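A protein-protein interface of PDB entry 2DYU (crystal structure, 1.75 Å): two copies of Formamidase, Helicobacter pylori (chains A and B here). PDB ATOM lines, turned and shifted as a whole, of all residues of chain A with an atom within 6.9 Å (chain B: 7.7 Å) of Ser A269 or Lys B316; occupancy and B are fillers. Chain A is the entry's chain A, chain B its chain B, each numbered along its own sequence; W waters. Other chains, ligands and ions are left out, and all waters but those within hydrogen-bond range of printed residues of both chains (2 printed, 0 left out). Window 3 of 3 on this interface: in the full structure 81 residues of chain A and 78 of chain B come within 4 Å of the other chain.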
ATOM      1  N   ASP A 264      14.839  19.518 -13.737  1.00  0.00           N
ATOM      2  CA  ASP A 264      14.890  20.979 -13.645  1.00  0.00           C
ATOM      3  C   ASP A 264      14.106  21.589 -14.804  1.00  0.00           C
ATOM      4  O   ASP A 264      13.311  22.509 -14.609  1.00  0.00           O
ATOM      5  CB  ASP A 264      16.334  21.489 -13.694  1.00  0.00           C
ATOM      6  CG  ASP A 264      17.153  21.090 -12.478  1.00  0.00           C
ATOM      7  OD1 ASP A 264      16.582  20.572 -11.490  1.00  0.00           O
ATOM      8  OD2 ASP A 264      18.381  21.322 -12.509  1.00  0.00           O
ATOM      9  N   ASN A 265      14.332  21.058 -16.008  1.00  0.00           N
ATOM     10  CA  ASN A 265      13.698  21.587 -17.224  1.00  0.00           C
ATOM     11  C   ASN A 265      12.191  21.368 -17.247  1.00  0.00           C
ATOM     12  O   ASN A 265      11.441  22.218 -17.725  1.00  0.00           O
ATOM     13  CB  ASN A 265      14.324  20.979 -18.482  1.00  0.00           C
ATOM     14  CG  ASN A 265      15.719  21.508 -18.766  1.00  0.00           C
ATOM     15  OD1 ASN A 265      16.138  22.530 -18.223  1.00  0.00           O
ATOM     16  ND2 ASN A 265      16.448  20.803 -19.631  1.00  0.00           N
ATOM     17  N   ALA A 266      11.745  20.227 -16.733  1.00  0.00           N
ATOM     18  CA  ALA A 266      10.325  19.981 -16.558  1.00  0.00           C
ATOM     19  C   ALA A 266       9.733  21.040 -15.629  1.00  0.00           C
ATOM     20  O   ALA A 266       8.687  21.618 -15.915  1.00  0.00           O
ATOM     21  CB  ALA A 266      10.094  18.583 -15.999  1.00  0.00           C
ATOM     22  N   ARG A 267      10.420  21.315 -14.522  1.00  0.00           N
ATOM     23  CA  ARG A 267       9.966  22.330 -13.570  1.00  0.00           C
ATOM     24  C   ARG A 267       9.900  23.744 -14.159  1.00  0.00           C
ATOM     25  O   ARG A 267       9.037  24.534 -13.778  1.00  0.00           O
ATOM     26  CB  ARG A 267      10.845  22.316 -12.323  1.00  0.00           C
ATOM     27  CG  ARG A 267      10.620  21.086 -11.452  1.00  0.00           C
ATOM     28  CD  ARG A 267      11.764  20.895 -10.498  1.00  0.00           C
ATOM     29  NE  ARG A 267      11.405  20.007  -9.399  1.00  0.00           N
ATOM     30  CZ  ARG A 267      12.193  19.778  -8.352  1.00  0.00           C
ATOM     31  NH1 ARG A 267      13.378  20.379  -8.270  1.00  0.00           N
ATOM     32  NH2 ARG A 267      11.795  18.960  -7.385  1.00  0.00           N
ATOM     33  N   LEU A 268      10.801  24.051 -15.086  1.00  0.00           N
ATOM     34  CA  LEU A 268      10.838  25.368 -15.721  1.00  0.00           C
ATOM     35  C   LEU A 268       9.824  25.507 -16.860  1.00  0.00           C
ATOM     36  O   LEU A 268       9.346  26.608 -17.134  1.00  0.00           O
ATOM     37  CB  LEU A 268      12.247  25.674 -16.254  1.00  0.00           C
ATOM     38  CG  LEU A 268      13.433  25.783 -15.289  1.00  0.00           C
ATOM     39  CD1 LEU A 268      14.704  26.116 -16.055  1.00  0.00           C
ATOM     40  CD2 LEU A 268      13.197  26.808 -14.201  1.00  0.00           C
ATOM     41  N   SER A 269       9.502  24.397 -17.524  1.00  0.00           N
ATOM     42  CA  SER A 269       8.770  24.452 -18.797  1.00  0.00           C
ATOM     43  C   SER A 269       7.327  23.966 -18.755  1.00  0.00           C
ATOM     44  O   SER A 269       6.482  24.442 -19.523  1.00  0.00           O
ATOM     45  CB  SER A 269       9.514  23.657 -19.870  1.00  0.00           C
ATOM     46  OG  SER A 269      10.826  24.147 -20.051  1.00  0.00           O
ATOM     47  N   TRP A 270       7.050  23.001 -17.888  1.00  0.00           N
ATOM     48  CA  TRP A 270       5.743  22.358 -17.873  1.00  0.00           C
ATOM     49  C   TRP A 270       4.651  23.274 -17.323  1.00  0.00           C
ATOM     50  O   TRP A 270       4.913  24.121 -16.461  1.00  0.00           O
ATOM     51  CB  TRP A 270       5.812  21.020 -17.125  1.00  0.00           C
ATOM     52  CG  TRP A 270       6.394  19.914 -17.968  1.00  0.00           C
ATOM     53  CD1 TRP A 270       6.892  20.030 -19.236  1.00  0.00           C
ATOM     54  CD2 TRP A 270       6.558  18.534 -17.600  1.00  0.00           C
ATOM     55  NE1 TRP A 270       7.339  18.809 -19.685  1.00  0.00           N
ATOM     56  CE2 TRP A 270       7.145  17.875 -18.702  1.00  0.00           C
ATOM     57  CE3 TRP A 270       6.256  17.792 -16.455  1.00  0.00           C
ATOM     58  CZ2 TRP A 270       7.442  16.511 -18.687  1.00  0.00           C
ATOM     59  CZ3 TRP A 270       6.548  16.431 -16.445  1.00  0.00           C
ATOM     60  CH2 TRP A 270       7.136  15.808 -17.554  1.00  0.00           C
ATOM     61  N   GLY A 271       3.437  23.114 -17.850  1.00  0.00           N
ATOM     62  CA  GLY A 271       2.290  23.918 -17.433  1.00  0.00           C
ATOM     63  C   GLY A 271       1.328  23.133 -16.557  1.00  0.00           C
ATOM     64  O   GLY A 271       1.400  23.203 -15.332  1.00  0.00           O
ATOM     65  N   LEU A 272       0.430  22.377 -17.184  1.00  0.00           N
ATOM     66  CA  LEU A 272      -0.553  21.573 -16.455  1.00  0.00           C
ATOM     67  C   LEU A 272       0.090  20.605 -15.460  1.00  0.00           C
ATOM     68  O   LEU A 272      -0.463  20.343 -14.389  1.00  0.00           O
ATOM     69  CB  LEU A 272      -1.439  20.800 -17.439  1.00  0.00           C
ATOM     70  CG  LEU A 272      -2.258  21.695 -18.373  1.00  0.00           C
ATOM     71  CD1 LEU A 272      -2.838  20.917 -19.559  1.00  0.00           C
ATOM     72  CD2 LEU A 272      -3.356  22.367 -17.583  1.00  0.00           C
ATOM     73  N   GLU A 273       1.260  20.083 -15.818  1.00  0.00           N
ATOM     74  CA  GLU A 273       1.959  19.114 -14.975  1.00  0.00           C
ATOM     75  C   GLU A 273       2.686  19.767 -13.807  1.00  0.00           C
ATOM     76  O   GLU A 273       3.176  19.075 -12.912  1.00  0.00           O
ATOM     77  CB  GLU A 273       2.967  18.311 -15.802  1.00  0.00           C
ATOM     78  CG  GLU A 273       2.371  17.573 -16.983  1.00  0.00           C
ATOM     79  CD  GLU A 273       2.281  18.431 -18.236  1.00  0.00           C
ATOM     80  OE1 GLU A 273       2.397  19.672 -18.139  1.00  0.00           O
ATOM     81  OE2 GLU A 273       2.090  17.854 -19.325  1.00  0.00           O
ATOM     82  N   ASN A 274       2.745  21.095 -13.813  1.00  0.00           N
ATOM     83  CA  ASN A 274       3.558  21.825 -12.851  1.00  0.00           C
ATOM     84  C   ASN A 274       2.827  22.081 -11.543  1.00  0.00           C
ATOM     85  O   ASN A 274       2.625  23.230 -11.143  1.00  0.00           O
ATOM     86  CB  ASN A 274       4.039  23.146 -13.454  1.00  0.00           C
ATOM     87  CG  ASN A 274       5.443  23.495 -13.023  1.00  0.00           C
ATOM     88  OD1 ASN A 274       5.825  23.272 -11.873  1.00  0.00           O
ATOM     89  ND2 ASN A 274       6.228  24.036 -13.951  1.00  0.00           N
ATOM     90  N   TRP B 311      13.555  28.353  -8.312  1.00  0.00           N
ATOM     91  CA  TRP B 311      13.759  28.478  -9.755  1.00  0.00           C
ATOM     92  C   TRP B 311      12.709  29.351 -10.449  1.00  0.00           C
ATOM     93  O   TRP B 311      12.656  29.398 -11.677  1.00  0.00           O
ATOM     94  CB  TRP B 311      13.764  27.091 -10.402  1.00  0.00           C
ATOM     95  CG  TRP B 311      12.531  26.280 -10.097  1.00  0.00           C
ATOM     96  CD1 TRP B 311      11.314  26.365 -10.718  1.00  0.00           C
ATOM     97  CD2 TRP B 311      12.399  25.259  -9.098  1.00  0.00           C
ATOM     98  NE1 TRP B 311      10.434  25.465 -10.162  1.00  0.00           N
ATOM     99  CE2 TRP B 311      11.076  24.774  -9.167  1.00  0.00           C
ATOM    100  CE3 TRP B 311      13.271  24.712  -8.147  1.00  0.00           C
ATOM    101  CZ2 TRP B 311      10.605  23.761  -8.325  1.00  0.00           C
ATOM    102  CZ3 TRP B 311      12.799  23.706  -7.310  1.00  0.00           C
ATOM    103  CH2 TRP B 311      11.479  23.243  -7.406  1.00  0.00           C
ATOM    104  N   GLU B 312      11.879  30.036  -9.666  1.00  0.00           N
ATOM    105  CA  GLU B 312      10.752  30.794 -10.222  1.00  0.00           C
ATOM    106  C   GLU B 312      11.124  31.899 -11.208  1.00  0.00           C
ATOM    107  O   GLU B 312      10.345  32.214 -12.109  1.00  0.00           O
ATOM    108  CB  GLU B 312       9.900  31.382  -9.105  1.00  0.00           C
ATOM    109  CG  GLU B 312       8.852  30.430  -8.601  1.00  0.00           C
ATOM    110  CD  GLU B 312       7.909  31.075  -7.615  1.00  0.00           C
ATOM    111  OE1 GLU B 312       7.630  32.287  -7.752  1.00  0.00           O
ATOM    112  OE2 GLU B 312       7.441  30.365  -6.709  1.00  0.00           O
ATOM    113  N   ASP B 313      12.304  32.485 -11.037  1.00  0.00           N
ATOM    114  CA  ASP B 313      12.750  33.568 -11.910  1.00  0.00           C
ATOM    115  C   ASP B 313      13.333  33.070 -13.230  1.00  0.00           C
ATOM    116  O   ASP B 313      13.884  33.855 -14.002  1.00  0.00           O
ATOM    117  CB  ASP B 313      13.783  34.441 -11.196  1.00  0.00           C
ATOM    118  CG  ASP B 313      13.237  35.080  -9.935  1.00  0.00           C
ATOM    119  OD1 ASP B 313      12.008  35.295  -9.852  1.00  0.00           O
ATOM    120  OD2 ASP B 313      14.045  35.370  -9.029  1.00  0.00           O
ATOM    121  N   HIS B 314      13.216  31.774 -13.494  1.00  0.00           N
ATOM    122  CA  HIS B 314      13.754  31.213 -14.728  1.00  0.00           C
ATOM    123  C   HIS B 314      12.729  30.386 -15.499  1.00  0.00           C
ATOM    124  O   HIS B 314      13.084  29.629 -16.398  1.00  0.00           O
ATOM    125  CB  HIS B 314      14.997  30.373 -14.433  1.00  0.00           C
ATOM    126  CG  HIS B 314      16.166  31.172 -13.946  1.00  0.00           C
ATOM    127  ND1 HIS B 314      16.822  32.089 -14.738  1.00  0.00           N
ATOM    128  CD2 HIS B 314      16.804  31.182 -12.751  1.00  0.00           C
ATOM    129  CE1 HIS B 314      17.812  32.633 -14.052  1.00  0.00           C
ATOM    130  NE2 HIS B 314      17.824  32.099 -12.844  1.00  0.00           N
ATOM    131  N   MET B 315      11.456  30.551 -15.158  1.00  0.00           N
ATOM    132  CA  MET B 315      10.401  29.723 -15.736  1.00  0.00           C
ATOM    133  C   MET B 315       9.845  30.250 -17.057  1.00  0.00           C
ATOM    134  O   MET B 315       9.947  31.439 -17.358  1.00  0.00           O
ATOM    135  CB  MET B 315       9.270  29.527 -14.728  1.00  0.00           C
ATOM    136  CG  MET B 315       9.638  28.602 -13.583  1.00  0.00           C
ATOM    137  SD  MET B 315       8.271  28.357 -12.447  1.00  0.00           S
ATOM    138  CE  MET B 315       7.060  27.591 -13.525  1.00  0.00           C
ATOM    139  N   LYS B 316       9.254  29.347 -17.836  1.00  0.00           N
ATOM    140  CA  LYS B 316       8.641  29.693 -19.116  1.00  0.00           C
ATOM    141  C   LYS B 316       7.131  29.909 -18.986  1.00  0.00           C
ATOM    142  O   LYS B 316       6.651  31.041 -19.085  1.00  0.00           O
ATOM    143  CB  LYS B 316       8.925  28.611 -20.161  1.00  0.00           C
ATOM    144  CG  LYS B 316      10.394  28.414 -20.490  1.00  0.00           C
ATOM    145  CD  LYS B 316      10.561  27.324 -21.541  1.00  0.00           C
ATOM    146  CE  LYS B 316      12.023  27.062 -21.861  1.00  0.00           C
ATOM    147  NZ  LYS B 316      12.179  25.874 -22.753  1.00  0.00           N
ATOM    148  N   ILE B 317       6.388  28.824 -18.769  1.00  0.00           N
ATOM    149  CA  ILE B 317       4.930  28.899 -18.648  1.00  0.00           C
ATOM    150  C   ILE B 317       4.503  29.511 -17.312  1.00  0.00           C
ATOM    151  O   ILE B 317       4.649  28.891 -16.253  1.00  0.00           O
ATOM    152  CB  ILE B 317       4.248  27.516 -18.847  1.00  0.00           C
ATOM    153  CG1 ILE B 317       4.441  27.027 -20.285  1.00  0.00           C
ATOM    154  CG2 ILE B 317       2.758  27.594 -18.522  1.00  0.00           C
ATOM    155  CD1 ILE B 317       3.676  25.755 -20.617  1.00  0.00           C
ATOM    156  N   LYS B 318       3.987  30.738 -17.377  1.00  0.00           N
ATOM    157  CA  LYS B 318       3.498  31.447 -16.196  1.00  0.00           C
ATOM    158  C   LYS B 318       2.251  32.286 -16.498  1.00  0.00           C
ATOM    159  O   LYS B 318       1.652  32.865 -15.590  1.00  0.00           O
ATOM    160  CB  LYS B 318       4.600  32.322 -15.582  1.00  0.00           C
ATOM    161  CG  LYS B 318       5.572  31.566 -14.682  1.00  0.00           C
ATOM    162  CD  LYS B 318       6.482  32.507 -13.904  1.00  0.00           C
ATOM    163  CE  LYS B 318       7.526  33.156 -14.801  1.00  0.00           C
ATOM    164  NZ  LYS B 318       8.510  33.949 -14.011  1.00  0.00           N
ATOM    165  N   ASP B 319       1.876  32.355 -17.775  1.00  0.00           N
ATOM    166  CA  ASP B 319       0.623  32.997 -18.191  1.00  0.00           C
ATOM    167  C   ASP B 319       0.040  32.311 -19.430  1.00  0.00           C
ATOM    168  O   ASP B 319       0.764  31.655 -20.184  1.00  0.00           O
ATOM    169  CB  ASP B 319       0.800  34.509 -18.405  1.00  0.00           C
ATOM    170  CG  ASP B 319       1.640  34.843 -19.626  1.00  0.00           C
ATOM    171  OD1 ASP B 319       1.093  34.843 -20.750  1.00  0.00           O
ATOM    172  OD2 ASP B 319       2.843  35.136 -19.459  1.00  0.00           O
ATOM    173  N   ILE B 322      -0.361  31.198 -24.471  1.00  0.00           N
ATOM    174  CA  ILE B 322       0.034  30.101 -25.356  1.00  0.00           C
ATOM    175  C   ILE B 322      -1.197  29.507 -26.056  1.00  0.00           C
ATOM    176  O   ILE B 322      -1.078  28.692 -26.975  1.00  0.00           O
ATOM    177  CB  ILE B 322       0.837  29.012 -24.590  1.00  0.00           C
ATOM    178  CG1 ILE B 322       1.713  28.196 -25.549  1.00  0.00           C
ATOM    179  CG2 ILE B 322      -0.093  28.129 -23.754  1.00  0.00           C
ATOM    180  CD1 ILE B 322       2.734  27.314 -24.857  1.00  0.00           C
HETATM  181  O   HOH W   1       7.989  24.437 -11.126  1.00  0.00           O
HETATM  182  O   HOH W   2      13.675  23.409 -21.329  1.00  0.00           O
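N of Lys B316 sits at hydrogen-bond distance from O of Leu A268, 2.8 Å away.
OG of Ser A269 lies within hydrogen-bond range of NZ of Lys B316 (3.5 Å).
OG of Ser A269 sits at hydrogen-bond distance from O of Asn A265, 3.1 Å away.
The side-chain amide nitrogen (ND2) of Asn A274 sits at hydrogen-bond distance from the backbone carbonyl oxygen (O) of Arg A267 (2.9 Å).
The backbone carbonyl oxygen of Trp A270 sits at hydrogen-bond distance from the side-chain amide nitrogen of Asn A274, at 2.8 Å.
Among the printed residues, pairs that only touch across the chains: Ser A269 with Ile B317 (3.3 Å), Arg A267 with Trp B311 (3.5 Å), Leu A268 with Met B315 (3.6 Å), Leu A268 with His B314 (3.6 Å), Arg A267 with Met B315 (3.6 Å), Leu A268 with Trp B311 (3.7 Å), Asn A274 with Met B315 (3.7 Å) and Gly A271 with Ile B317 (3.8 Å).
Asp A264 touches none of the printed residues of chain B.
Ser A269 touches just these residues of chain B: Lys B316 and Ile B317.
Of the printed residues of chain A, Trp B311 touches Arg A267 and Leu A268.
Glu B312 touches none of the printed residues of chain A.
Printed residues of chain A within 4 Å of His B314: Leu A268 (3.6 Å).
Of chain A, only Leu A268 (2.8 Å) and Ser A269 (3.5 Å) come within 4 Å of Lys B316.
Of the printed residues of chain A, Ile B317 touches Ser A269 (3.3 Å) and Gly A271 (3.8 Å).
The nearest printed residue of chain A that does not touch His B314 is Ser A269 (6.4 Å).
Hydrophobic or aromatic side chains of chain A that line the printed part of chain B: Leu A268.
Printed residues of chain B that touch a printed residue of chain A: Trp B311, His B314, Met B315, Lys B316 and Ile B317.
Hydrophobic or aromatic side chains of chain B that line the printed part of chain A: Trp B311, Met B315 and Ile B317.
No position is printed for both chains.
Of the 10 pairs that touch across the chains among the printed residues, none has its exchanged pair printed and touching as well.
Water W1 lies within hydrogen-bond range of the side-chain amide oxygen of Asn A274 (2.6 Å), the indole nitrogen of Trp B311 (2.8 Å) and the backbone carbonyl oxygen of Arg A267 (2.9 Å).
Water W2 lies within hydrogen-bond range of OG of Ser A269 (3.2 Å) and NZ of Lys B316 (3.2 Å).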
